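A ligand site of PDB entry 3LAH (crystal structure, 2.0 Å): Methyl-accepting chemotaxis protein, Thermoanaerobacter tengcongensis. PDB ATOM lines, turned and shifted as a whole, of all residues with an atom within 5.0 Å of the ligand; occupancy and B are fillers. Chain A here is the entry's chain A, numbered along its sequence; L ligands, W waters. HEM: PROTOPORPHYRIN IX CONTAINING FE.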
ATOM      1  N   MET A   1      -0.064   8.789  15.088  1.00  0.00           N
ATOM      2  CA  MET A   1      -0.986   9.639  14.349  1.00  0.00           C
ATOM      3  C   MET A   1      -2.068  10.220  15.254  1.00  0.00           C
ATOM      4  O   MET A   1      -2.488   9.571  16.211  1.00  0.00           O
ATOM      5  CB  MET A   1      -1.669   8.851  13.229  1.00  0.00           C
ATOM      6  CG  MET A   1      -0.716   8.191  12.259  1.00  0.00           C
ATOM      7  SD  MET A   1       0.295   9.385  11.377  1.00  0.00           S
ATOM      8  CE  MET A   1       0.862   8.359  10.020  1.00  0.00           C
ATOM      9  N   LYS A   2      -2.505  11.434  14.941  1.00  0.00           N
ATOM     10  CA  LYS A   2      -3.657  12.006  15.608  1.00  0.00           C
ATOM     11  C   LYS A   2      -4.927  11.244  15.221  1.00  0.00           C
ATOM     12  O   LYS A   2      -5.036  10.718  14.117  1.00  0.00           O
ATOM     13  CB  LYS A   2      -3.793  13.491  15.260  1.00  0.00           C
ATOM     14  CG  LYS A   2      -2.898  14.389  16.089  1.00  0.00           C
ATOM     15  CD  LYS A   2      -3.379  14.425  17.533  1.00  0.00           C
ATOM     16  CE  LYS A   2      -2.498  15.303  18.397  1.00  0.00           C
ATOM     17  NZ  LYS A   2      -3.093  15.557  19.743  1.00  0.00           N
ATOM     18  N   THR A   4      -7.910  11.966  14.323  1.00  0.00           N
ATOM     19  CA  THR A   4      -8.716  12.354  13.172  1.00  0.00           C
ATOM     20  C   THR A   4      -8.369  11.502  11.948  1.00  0.00           C
ATOM     21  O   THR A   4      -9.237  10.861  11.361  1.00  0.00           O
ATOM     22  CB  THR A   4      -8.534  13.848  12.813  1.00  0.00           C
ATOM     23  OG1 THR A   4      -7.196  14.060  12.348  1.00  0.00           O
ATOM     24  CG2 THR A   4      -8.782  14.706  14.031  1.00  0.00           C
ATOM     25  N   ILE A   5      -7.102  11.479  11.589  1.00  0.00           N
ATOM     26  CA  ILE A   5      -6.677  10.753  10.402  1.00  0.00           C
ATOM     27  C   ILE A   5      -6.885   9.247  10.561  1.00  0.00           C
ATOM     28  O   ILE A   5      -7.403   8.590   9.662  1.00  0.00           O
ATOM     29  CB  ILE A   5      -5.218  11.070  10.035  1.00  0.00           C
ATOM     30  CG1 ILE A   5      -4.867  10.443   8.683  1.00  0.00           C
ATOM     31  CG2 ILE A   5      -4.268  10.602  11.126  1.00  0.00           C
ATOM     32  CD1 ILE A   5      -3.718  11.143   7.987  1.00  0.00           C
ATOM     33  N   TRP A   9      -8.984   6.370   8.273  1.00  0.00           N
ATOM     34  CA  TRP A   9      -8.376   5.141   7.764  1.00  0.00           C
ATOM     35  C   TRP A   9      -9.256   3.920   8.043  1.00  0.00           C
ATOM     36  O   TRP A   9      -9.416   3.048   7.186  1.00  0.00           O
ATOM     37  CB  TRP A   9      -6.970   4.913   8.328  1.00  0.00           C
ATOM     38  CG  TRP A   9      -5.942   5.893   7.825  1.00  0.00           C
ATOM     39  CD1 TRP A   9      -6.036   6.694   6.722  1.00  0.00           C
ATOM     40  CD2 TRP A   9      -4.650   6.148   8.398  1.00  0.00           C
ATOM     41  NE1 TRP A   9      -4.893   7.448   6.577  1.00  0.00           N
ATOM     42  CE2 TRP A   9      -4.031   7.137   7.599  1.00  0.00           C
ATOM     43  CE3 TRP A   9      -3.965   5.666   9.510  1.00  0.00           C
ATOM     44  CZ2 TRP A   9      -2.755   7.634   7.866  1.00  0.00           C
ATOM     45  CZ3 TRP A   9      -2.698   6.153   9.782  1.00  0.00           C
ATOM     46  CH2 TRP A   9      -2.103   7.131   8.962  1.00  0.00           C
ATOM     47  N   ILE A  75      -9.303  10.178   0.188  1.00  0.00           N
ATOM     48  CA  ILE A  75      -9.646  11.523  -0.224  1.00  0.00           C
ATOM     49  C   ILE A  75     -11.164  11.704  -0.166  1.00  0.00           C
ATOM     50  O   ILE A  75     -11.660  12.723   0.321  1.00  0.00           O
ATOM     51  CB  ILE A  75      -9.118  11.865  -1.637  1.00  0.00           C
ATOM     52  CG1 ILE A  75      -7.597  12.044  -1.602  1.00  0.00           C
ATOM     53  CG2 ILE A  75      -9.761  13.137  -2.176  1.00  0.00           C
ATOM     54  CD1 ILE A  75      -7.147  13.219  -0.742  1.00  0.00           C
ATOM     55  N   PHE A  78     -12.186  11.772   3.596  1.00  0.00           N
ATOM     56  CA  PHE A  78     -11.793  13.038   4.207  1.00  0.00           C
ATOM     57  C   PHE A  78     -12.674  14.165   3.714  1.00  0.00           C
ATOM     58  O   PHE A  78     -13.060  15.047   4.477  1.00  0.00           O
ATOM     59  CB  PHE A  78     -10.329  13.346   3.872  1.00  0.00           C
ATOM     60  CG  PHE A  78      -9.623  14.177   4.899  1.00  0.00           C
ATOM     61  CD1 PHE A  78      -9.085  13.595   6.031  1.00  0.00           C
ATOM     62  CD2 PHE A  78      -9.475  15.551   4.724  1.00  0.00           C
ATOM     63  CE1 PHE A  78      -8.427  14.353   6.973  1.00  0.00           C
ATOM     64  CE2 PHE A  78      -8.817  16.315   5.659  1.00  0.00           C
ATOM     65  CZ  PHE A  78      -8.284  15.716   6.790  1.00  0.00           C
ATOM     66  N   TYR A  85     -12.074  22.051   3.090  1.00  0.00           N
ATOM     67  CA  TYR A  85     -10.787  22.060   2.400  1.00  0.00           C
ATOM     68  C   TYR A  85     -10.941  21.812   0.903  1.00  0.00           C
ATOM     69  O   TYR A  85      -9.996  22.015   0.141  1.00  0.00           O
ATOM     70  CB  TYR A  85      -9.852  21.010   2.994  1.00  0.00           C
ATOM     71  CG  TYR A  85      -9.457  21.257   4.420  1.00  0.00           C
ATOM     72  CD1 TYR A  85     -10.147  20.648   5.466  1.00  0.00           C
ATOM     73  CD2 TYR A  85      -8.373  22.073   4.743  1.00  0.00           C
ATOM     74  CE1 TYR A  85      -9.785  20.866   6.779  1.00  0.00           C
ATOM     75  CE2 TYR A  85      -8.002  22.294   6.059  1.00  0.00           C
ATOM     76  CZ  TYR A  85      -8.706  21.690   7.070  1.00  0.00           C
ATOM     77  OH  TYR A  85      -8.349  21.891   8.382  1.00  0.00           O
ATOM     78  N   PHE A  86     -12.118  21.379   0.484  1.00  0.00           N
ATOM     79  CA  PHE A  86     -12.373  21.045  -0.905  1.00  0.00           C
ATOM     80  C   PHE A  86     -13.352  22.002  -1.574  1.00  0.00           C
ATOM     81  O   PHE A  86     -13.287  22.241  -2.784  1.00  0.00           O
ATOM     82  CB  PHE A  86     -12.911  19.618  -1.022  1.00  0.00           C
ATOM     83  CG  PHE A  86     -12.007  18.584  -0.417  1.00  0.00           C
ATOM     84  CD1 PHE A  86     -11.187  17.804  -1.205  1.00  0.00           C
ATOM     85  CD2 PHE A  86     -11.983  18.391   0.960  1.00  0.00           C
ATOM     86  CE1 PHE A  86     -10.361  16.843  -0.645  1.00  0.00           C
ATOM     87  CE2 PHE A  86     -11.162  17.438   1.526  1.00  0.00           C
ATOM     88  CZ  PHE A  86     -10.341  16.670   0.722  1.00  0.00           C
ATOM     89  N   PHE A  94      -5.646  23.503  -4.778  1.00  0.00           N
ATOM     90  CA  PHE A  94      -5.719  22.549  -3.673  1.00  0.00           C
ATOM     91  C   PHE A  94      -4.352  21.958  -3.369  1.00  0.00           C
ATOM     92  O   PHE A  94      -3.918  21.915  -2.222  1.00  0.00           O
ATOM     93  CB  PHE A  94      -6.733  21.458  -4.020  1.00  0.00           C
ATOM     94  CG  PHE A  94      -6.844  20.366  -2.998  1.00  0.00           C
ATOM     95  CD1 PHE A  94      -7.696  20.502  -1.904  1.00  0.00           C
ATOM     96  CD2 PHE A  94      -6.128  19.179  -3.141  1.00  0.00           C
ATOM     97  CE1 PHE A  94      -7.813  19.481  -0.979  1.00  0.00           C
ATOM     98  CE2 PHE A  94      -6.245  18.158  -2.216  1.00  0.00           C
ATOM     99  CZ  PHE A  94      -7.088  18.309  -1.135  1.00  0.00           C
ATOM    100  N   LEU A  95      -3.651  21.517  -4.414  1.00  0.00           N
ATOM    101  CA  LEU A  95      -2.354  20.885  -4.234  1.00  0.00           C
ATOM    102  C   LEU A  95      -1.289  21.866  -3.743  1.00  0.00           C
ATOM    103  O   LEU A  95      -0.484  21.533  -2.880  1.00  0.00           O
ATOM    104  CB  LEU A  95      -1.898  20.195  -5.532  1.00  0.00           C
ATOM    105  CG  LEU A  95      -2.699  18.959  -5.912  1.00  0.00           C
ATOM    106  CD1 LEU A  95      -2.313  18.450  -7.298  1.00  0.00           C
ATOM    107  CD2 LEU A  95      -2.496  17.866  -4.872  1.00  0.00           C
ATOM    108  N   MET A  98      -1.489  22.990   0.054  1.00  0.00           N
ATOM    109  CA  MET A  98      -1.498  21.951   1.082  1.00  0.00           C
ATOM    110  C   MET A  98      -0.301  21.990   2.043  1.00  0.00           C
ATOM    111  O   MET A  98      -0.427  21.602   3.186  1.00  0.00           O
ATOM    112  CB  MET A  98      -1.668  20.562   0.454  1.00  0.00           C
ATOM    113  CG  MET A  98      -2.402  19.582   1.372  1.00  0.00           C
ATOM    114  SD  MET A  98      -3.910  20.288   2.086  1.00  0.00           S
ATOM    115  CE  MET A  98      -5.025  20.186   0.695  1.00  0.00           C
ATOM    116  N   VAL A 101      -1.239  24.492   4.681  1.00  0.00           N
ATOM    117  CA  VAL A 101      -2.281  23.882   5.502  1.00  0.00           C
ATOM    118  C   VAL A 101      -1.666  23.010   6.599  1.00  0.00           C
ATOM    119  O   VAL A 101      -2.087  23.059   7.748  1.00  0.00           O
ATOM    120  CB  VAL A 101      -3.246  23.036   4.661  1.00  0.00           C
ATOM    121  CG1 VAL A 101      -4.149  22.189   5.552  1.00  0.00           C
ATOM    122  CG2 VAL A 101      -4.064  23.931   3.744  1.00  0.00           C
ATOM    123  N   LEU A 105      -1.781  23.626  10.558  1.00  0.00           N
ATOM    124  CA  LEU A 105      -2.261  22.510  11.373  1.00  0.00           C
ATOM    125  C   LEU A 105      -1.309  22.209  12.520  1.00  0.00           C
ATOM    126  O   LEU A 105      -1.730  22.039  13.663  1.00  0.00           O
ATOM    127  CB  LEU A 105      -2.432  21.272  10.496  1.00  0.00           C
ATOM    128  CG  LEU A 105      -3.469  21.260   9.368  1.00  0.00           C
ATOM    129  CD1 LEU A 105      -3.336  19.974   8.562  1.00  0.00           C
ATOM    130  CD2 LEU A 105      -4.885  21.409   9.901  1.00  0.00           C
ATOM    131  N   GLY A 111       1.087  18.185  18.838  1.00  0.00           N
ATOM    132  CA  GLY A 111       1.499  16.830  18.543  1.00  0.00           C
ATOM    133  C   GLY A 111       1.316  16.403  17.095  1.00  0.00           C
ATOM    134  O   GLY A 111       1.811  15.351  16.685  1.00  0.00           O
ATOM    135  N   ALA A 112       0.602  17.201  16.307  1.00  0.00           N
ATOM    136  CA  ALA A 112       0.360  16.869  14.907  1.00  0.00           C
ATOM    137  C   ALA A 112       1.625  17.040  14.064  1.00  0.00           C
ATOM    138  O   ALA A 112       2.347  18.022  14.192  1.00  0.00           O
ATOM    139  CB  ALA A 112      -0.770  17.725  14.347  1.00  0.00           C
ATOM    140  N   THR A 113       1.899  16.063  13.198  1.00  0.00           N
ATOM    141  CA  THR A 113       3.064  16.176  12.320  1.00  0.00           C
ATOM    142  C   THR A 113       2.765  15.790  10.876  1.00  0.00           C
ATOM    143  O   THR A 113       3.311  14.804  10.365  1.00  0.00           O
ATOM    144  CB  THR A 113       4.243  15.342  12.835  1.00  0.00           C
ATOM    145  OG1 THR A 113       3.824  13.998  13.039  1.00  0.00           O
ATOM    146  CG2 THR A 113       4.767  15.914  14.151  1.00  0.00           C
ATOM    147  N   PRO A 114       1.895  16.568  10.196  1.00  0.00           N
ATOM    148  CA  PRO A 114       1.636  16.375   8.765  1.00  0.00           C
ATOM    149  C   PRO A 114       2.926  16.580   7.987  1.00  0.00           C
ATOM    150  O   PRO A 114       3.717  17.456   8.338  1.00  0.00           O
ATOM    151  CB  PRO A 114       0.667  17.509   8.414  1.00  0.00           C
ATOM    152  CG  PRO A 114       0.179  18.064   9.720  1.00  0.00           C
ATOM    153  CD  PRO A 114       1.233  17.771  10.735  1.00  0.00           C
ATOM    154  N   PRO A 115       3.151  15.767   6.944  1.00  0.00           N
ATOM    155  CA  PRO A 115       4.393  15.883   6.172  1.00  0.00           C
ATOM    156  C   PRO A 115       4.471  17.214   5.427  1.00  0.00           C
ATOM    157  O   PRO A 115       3.438  17.845   5.175  1.00  0.00           O
ATOM    158  CB  PRO A 115       4.278  14.747   5.134  1.00  0.00           C
ATOM    159  CG  PRO A 115       3.156  13.900   5.575  1.00  0.00           C
ATOM    160  CD  PRO A 115       2.258  14.715   6.439  1.00  0.00           C
ATOM    161  N   LEU A 117       4.794  19.164   2.004  1.00  0.00           N
ATOM    162  CA  LEU A 117       4.371  18.888   0.632  1.00  0.00           C
ATOM    163  C   LEU A 117       4.719  20.072  -0.261  1.00  0.00           C
ATOM    164  O   LEU A 117       3.875  20.529  -1.028  1.00  0.00           O
ATOM    165  CB  LEU A 117       2.873  18.606   0.567  1.00  0.00           C
ATOM    166  CG  LEU A 117       2.348  17.483   1.466  1.00  0.00           C
ATOM    167  CD1 LEU A 117       0.833  17.504   1.589  1.00  0.00           C
ATOM    168  CD2 LEU A 117       2.812  16.137   0.912  1.00  0.00           C
ATOM    169  N   MET A 129       6.102  18.408  -6.661  1.00  0.00           N
ATOM    170  CA  MET A 129       5.747  18.356  -5.245  1.00  0.00           C
ATOM    171  C   MET A 129       6.634  17.331  -4.556  1.00  0.00           C
ATOM    172  O   MET A 129       6.830  16.218  -5.072  1.00  0.00           O
ATOM    173  CB  MET A 129       4.267  18.021  -5.084  1.00  0.00           C
ATOM    174  CG  MET A 129       3.818  17.865  -3.638  1.00  0.00           C
ATOM    175  SD  MET A 129       2.081  17.386  -3.481  1.00  0.00           S
ATOM    176  CE  MET A 129       1.296  18.993  -3.518  1.00  0.00           C
ATOM    177  N   TYR A 131       7.145  15.206  -1.114  1.00  0.00           N
ATOM    178  CA  TYR A 131       6.782  14.652   0.174  1.00  0.00           C
ATOM    179  C   TYR A 131       8.039  14.535   1.039  1.00  0.00           C
ATOM    180  O   TYR A 131       9.022  13.925   0.619  1.00  0.00           O
ATOM    181  CB  TYR A 131       6.156  13.280  -0.043  1.00  0.00           C
ATOM    182  CG  TYR A 131       5.976  12.404   1.186  1.00  0.00           C
ATOM    183  CD1 TYR A 131       4.875  12.557   2.021  1.00  0.00           C
ATOM    184  CD2 TYR A 131       6.872  11.380   1.468  1.00  0.00           C
ATOM    185  CE1 TYR A 131       4.697  11.744   3.134  1.00  0.00           C
ATOM    186  CE2 TYR A 131       6.707  10.563   2.579  1.00  0.00           C
ATOM    187  CZ  TYR A 131       5.612  10.745   3.398  1.00  0.00           C
ATOM    188  OH  TYR A 131       5.442   9.924   4.492  1.00  0.00           O
ATOM    189  N   SER A 133       8.970  13.564   5.096  1.00  0.00           N
ATOM    190  CA  SER A 133       8.398  13.059   6.327  1.00  0.00           C
ATOM    191  C   SER A 133       9.409  12.288   7.156  1.00  0.00           C
ATOM    192  O   SER A 133      10.496  11.955   6.688  1.00  0.00           O
ATOM    193  CB  SER A 133       7.225  12.137   6.021  1.00  0.00           C
ATOM    194  OG  SER A 133       6.631  11.658   7.221  1.00  0.00           O
ATOM    195  N   ARG A 135       8.074   9.554   8.333  1.00  0.00           N
ATOM    196  CA  ARG A 135       7.242   8.355   8.350  1.00  0.00           C
ATOM    197  C   ARG A 135       7.277   7.412   7.137  1.00  0.00           C
ATOM    198  O   ARG A 135       6.741   6.307   7.197  1.00  0.00           O
ATOM    199  CB  ARG A 135       5.787   8.728   8.638  1.00  0.00           C
ATOM    200  CG  ARG A 135       5.507   9.186  10.062  1.00  0.00           C
ATOM    201  CD  ARG A 135       4.028   9.083  10.355  1.00  0.00           C
ATOM    202  NE  ARG A 135       3.702   9.428  11.728  1.00  0.00           N
ATOM    203  CZ  ARG A 135       3.316  10.634  12.110  1.00  0.00           C
ATOM    204  NH1 ARG A 135       3.208  11.609  11.220  1.00  0.00           N
ATOM    205  NH2 ARG A 135       3.034  10.872  13.386  1.00  0.00           N
ATOM    206  N   MET A 137       5.571   7.136   4.080  1.00  0.00           N
ATOM    207  CA  MET A 137       4.309   6.597   3.590  1.00  0.00           C
ATOM    208  C   MET A 137       4.163   6.891   2.099  1.00  0.00           C
ATOM    209  O   MET A 137       3.229   7.574   1.674  1.00  0.00           O
ATOM    210  CB  MET A 137       3.140   7.153   4.409  1.00  0.00           C
ATOM    211  CG  MET A 137       3.273   6.863   5.903  1.00  0.00           C
ATOM    212  SD  MET A 137       1.843   7.338   6.920  1.00  0.00           S
ATOM    213  CE  MET A 137       0.601   6.242   6.232  1.00  0.00           C
ATOM    214  N   TYR A 140       0.877   5.793   0.116  1.00  0.00           N
ATOM    215  CA  TYR A 140      -0.260   6.582   0.586  1.00  0.00           C
ATOM    216  C   TYR A 140      -0.228   7.968  -0.066  1.00  0.00           C
ATOM    217  O   TYR A 140      -1.217   8.423  -0.633  1.00  0.00           O
ATOM    218  CB  TYR A 140      -0.218   6.689   2.110  1.00  0.00           C
ATOM    219  CG  TYR A 140      -1.416   7.361   2.740  1.00  0.00           C
ATOM    220  CD1 TYR A 140      -2.710   6.980   2.399  1.00  0.00           C
ATOM    221  CD2 TYR A 140      -1.253   8.370   3.692  1.00  0.00           C
ATOM    222  CE1 TYR A 140      -3.803   7.591   2.970  1.00  0.00           C
ATOM    223  CE2 TYR A 140      -2.355   8.989   4.282  1.00  0.00           C
ATOM    224  CZ  TYR A 140      -3.624   8.589   3.913  1.00  0.00           C
ATOM    225  OH  TYR A 140      -4.722   9.189   4.477  1.00  0.00           O
ATOM    226  N   PHE A 141       0.936   8.614  -0.002  1.00  0.00           N
ATOM    227  CA  PHE A 141       1.130   9.912  -0.656  1.00  0.00           C
ATOM    228  C   PHE A 141       0.702   9.864  -2.129  1.00  0.00           C
ATOM    229  O   PHE A 141      -0.079  10.693  -2.576  1.00  0.00           O
ATOM    230  CB  PHE A 141       2.595  10.349  -0.547  1.00  0.00           C
ATOM    231  CG  PHE A 141       2.934  11.541  -1.421  1.00  0.00           C
ATOM    232  CD1 PHE A 141       2.433  12.803  -1.125  1.00  0.00           C
ATOM    233  CD2 PHE A 141       3.777  11.396  -2.510  1.00  0.00           C
ATOM    234  CE1 PHE A 141       2.752  13.909  -1.940  1.00  0.00           C
ATOM    235  CE2 PHE A 141       4.104  12.482  -3.328  1.00  0.00           C
ATOM    236  CZ  PHE A 141       3.590  13.747  -3.029  1.00  0.00           C
ATOM    237  N   LEU A 144      -3.087   9.450  -2.463  1.00  0.00           N
ATOM    238  CA  LEU A 144      -3.822  10.682  -2.159  1.00  0.00           C
ATOM    239  C   LEU A 144      -3.849  11.627  -3.362  1.00  0.00           C
ATOM    240  O   LEU A 144      -4.879  12.245  -3.649  1.00  0.00           O
ATOM    241  CB  LEU A 144      -3.218  11.382  -0.931  1.00  0.00           C
ATOM    242  CG  LEU A 144      -3.306  10.651   0.414  1.00  0.00           C
ATOM    243  CD1 LEU A 144      -2.362  11.281   1.428  1.00  0.00           C
ATOM    244  CD2 LEU A 144      -4.733  10.641   0.947  1.00  0.00           C
ATOM    245  N   ILE A 145      -2.719  11.740  -4.051  1.00  0.00           N
ATOM    246  CA  ILE A 145      -2.649  12.540  -5.265  1.00  0.00           C
ATOM    247  C   ILE A 145      -3.646  12.054  -6.307  1.00  0.00           C
ATOM    248  O   ILE A 145      -4.375  12.858  -6.899  1.00  0.00           O
ATOM    249  CB  ILE A 145      -1.246  12.517  -5.863  1.00  0.00           C
ATOM    250  CG1 ILE A 145      -0.263  13.228  -4.924  1.00  0.00           C
ATOM    251  CG2 ILE A 145      -1.227  13.186  -7.233  1.00  0.00           C
ATOM    252  CD1 ILE A 145       1.173  13.094  -5.355  1.00  0.00           C
ATOM    253  N   SER A 148      -7.180  12.820  -5.234  1.00  0.00           N
ATOM    254  CA  SER A 148      -7.510  14.239  -5.409  1.00  0.00           C
ATOM    255  C   SER A 148      -7.942  14.512  -6.833  1.00  0.00           C
ATOM    256  O   SER A 148      -8.904  15.247  -7.078  1.00  0.00           O
ATOM    257  CB  SER A 148      -6.307  15.120  -5.045  1.00  0.00           C
ATOM    258  OG  SER A 148      -5.985  14.992  -3.674  1.00  0.00           O
HETATM  259  CHA HEM L   1      -1.090  13.273   7.380  1.00  0.00           C
HETATM  260  CHB HEM L   1      -4.092  17.103   7.225  1.00  0.00           C
HETATM  261  CHC HEM L   1      -4.526  16.607   2.419  1.00  0.00           C
HETATM  262  CHD HEM L   1      -0.491  13.973   2.584  1.00  0.00           C
HETATM  263  C1A HEM L   1      -1.940  14.290   7.769  1.00  0.00           C
HETATM  264  C2A HEM L   1      -2.376  14.592   9.117  1.00  0.00           C
HETATM  265  C3A HEM L   1      -3.203  15.638   9.057  1.00  0.00           C
HETATM  266  C4A HEM L   1      -3.315  16.058   7.679  1.00  0.00           C
HETATM  267  CMA HEM L   1      -3.898  16.290  10.281  1.00  0.00           C
HETATM  268  CAA HEM L   1      -2.013  13.854  10.428  1.00  0.00           C
HETATM  269  CBA HEM L   1      -0.624  14.189  10.952  1.00  0.00           C
HETATM  270  CGA HEM L   1      -0.479  13.577  12.333  1.00  0.00           C
HETATM  271  O1A HEM L   1       0.584  13.799  12.976  1.00  0.00           O
HETATM  272  O2A HEM L   1      -1.404  12.856  12.775  1.00  0.00           O
HETATM  273  C1B HEM L   1      -4.560  17.245   5.926  1.00  0.00           C
HETATM  274  C2B HEM L   1      -5.686  18.060   5.474  1.00  0.00           C
HETATM  275  C3B HEM L   1      -5.763  17.924   4.142  1.00  0.00           C
HETATM  276  C4B HEM L   1      -4.739  17.004   3.720  1.00  0.00           C
HETATM  277  CMB HEM L   1      -6.577  18.945   6.380  1.00  0.00           C
HETATM  278  CAB HEM L   1      -6.761  18.508   3.116  1.00  0.00           C
HETATM  279  CBB HEM L   1      -8.074  18.524   3.341  1.00  0.00           C
HETATM  280  C1C HEM L   1      -3.403  15.916   2.026  1.00  0.00           C
HETATM  281  C2C HEM L   1      -2.941  15.733   0.670  1.00  0.00           C
HETATM  282  C3C HEM L   1      -1.820  14.989   0.720  1.00  0.00           C
HETATM  283  C4C HEM L   1      -1.545  14.700   2.103  1.00  0.00           C
HETATM  284  CMC HEM L   1      -3.654  16.312  -0.570  1.00  0.00           C
HETATM  285  CAC HEM L   1      -0.919  14.526  -0.453  1.00  0.00           C
HETATM  286  CBC HEM L   1      -1.026  15.055  -1.681  1.00  0.00           C
HETATM  287  C1D HEM L   1      -0.417  13.399   3.827  1.00  0.00           C
HETATM  288  C2D HEM L   1       0.269  12.162   4.103  1.00  0.00           C
HETATM  289  C3D HEM L   1       0.105  11.928   5.609  1.00  0.00           C
HETATM  290  C4D HEM L   1      -0.687  13.052   6.082  1.00  0.00           C
HETATM  291  CMD HEM L   1       1.021  11.288   3.062  1.00  0.00           C
HETATM  292  CAD HEM L   1       0.663  10.712   6.408  1.00  0.00           C
HETATM  293  CBD HEM L   1       1.699  11.181   7.411  1.00  0.00           C
HETATM  294  CGD HEM L   1       3.080  11.062   6.813  1.00  0.00           C
HETATM  295  O1D HEM L   1       3.222  10.409   5.754  1.00  0.00           O
HETATM  296  O2D HEM L   1       4.040  11.632   7.398  1.00  0.00           O
HETATM  297  NA  HEM L   1      -2.534  15.210   6.914  1.00  0.00           N
HETATM  298  NB  HEM L   1      -4.010  16.616   4.832  1.00  0.00           N
HETATM  299  NC  HEM L   1      -2.530  15.272   2.876  1.00  0.00           N
HETATM  300  ND  HEM L   1      -0.968  13.892   5.006  1.00  0.00           N
HETATM  301 FE   HEM L   1      -2.553  15.229   4.904  1.00  0.00          FE
HETATM  302  O   HOH W   1       1.070  12.782  15.204  1.00  0.00           O
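O2D of the ligand lies within hydrogen-bond range of OG of Ser 133, 2.6 Å away. OH of Tyr 131 sits at hydrogen-bond distance from O1D of the ligand. O1A of the ligand lies within hydrogen-bond range of N of Thr 113 (2.6 Å). An oxygen (O1A) of the ligand sits at hydrogen-bond distance from the side-chain hydroxyl of Thr 113, 3.2 Å away. N of Lys 2 sits at hydrogen-bond distance from O2A of the ligand (2.8 Å). NH2 of Arg 135 lies within salt-bridge range of O1A of the ligand (3.8 Å).
The side-chain hydroxyl of Ser 133 lies close to the side-chain hydroxyl of Tyr 131, 3.4 Å away. The backbone NH (N) of Arg 135 is in hydrogen-bond range of the side-chain hydroxyl (OG) of Ser 133 (2.8 Å). OH of Tyr 131 sits at hydrogen-bond distance from N of Met 137. The side-chain hydroxyl (OG1) of Thr 113 is in hydrogen-bond range of the guanidinium group (NH1) of Arg 135 (3.1 Å). The backbone carbonyl oxygen (O) of Leu 144 lies within hydrogen-bond range of the side-chain hydroxyl (OG) of Ser 148, 3.0 Å away. The side-chain sulfur of Met 1 sits close to the guanidinium group of Arg 135, at 3.4 Å. OH of Tyr 140 sits at hydrogen-bond distance from NE1 of Trp 9 (2.7 Å).
The side-chain sulfur (SD) of Met 137 sits close to an oxygen (O1D) of the ligand (3.6 Å). Merely in contact with the ligand: Pro 115 (3.0 Å), Tyr 85 (3.1 Å), Leu 105 (3.3 Å), Phe 78 (3.3 Å), Met 98 (3.4 Å), Ile 5 (3.4 Å), Leu 144 (3.5 Å), Pro 114 (3.5 Å), Ala 112 (3.6 Å), Phe 94 (3.6 Å), Met 1 (3.6 Å), Leu 117 (3.7 Å), Phe 86 (3.7 Å), Tyr 140 (3.8 Å), Ile 145 (3.8 Å) and Phe 141 (3.8 Å). Along chain A the residues within 4 Å of the ligand span positions 1 to 145. The nearest printed residue that does not touch the ligand is Ser 148 (4.1 Å).
Water W1 lies within hydrogen-bond range of O1A of the ligand (2.5 Å), O of Gly 111 (3.1 Å) and NH2 of Arg 135 (3.3 Å).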
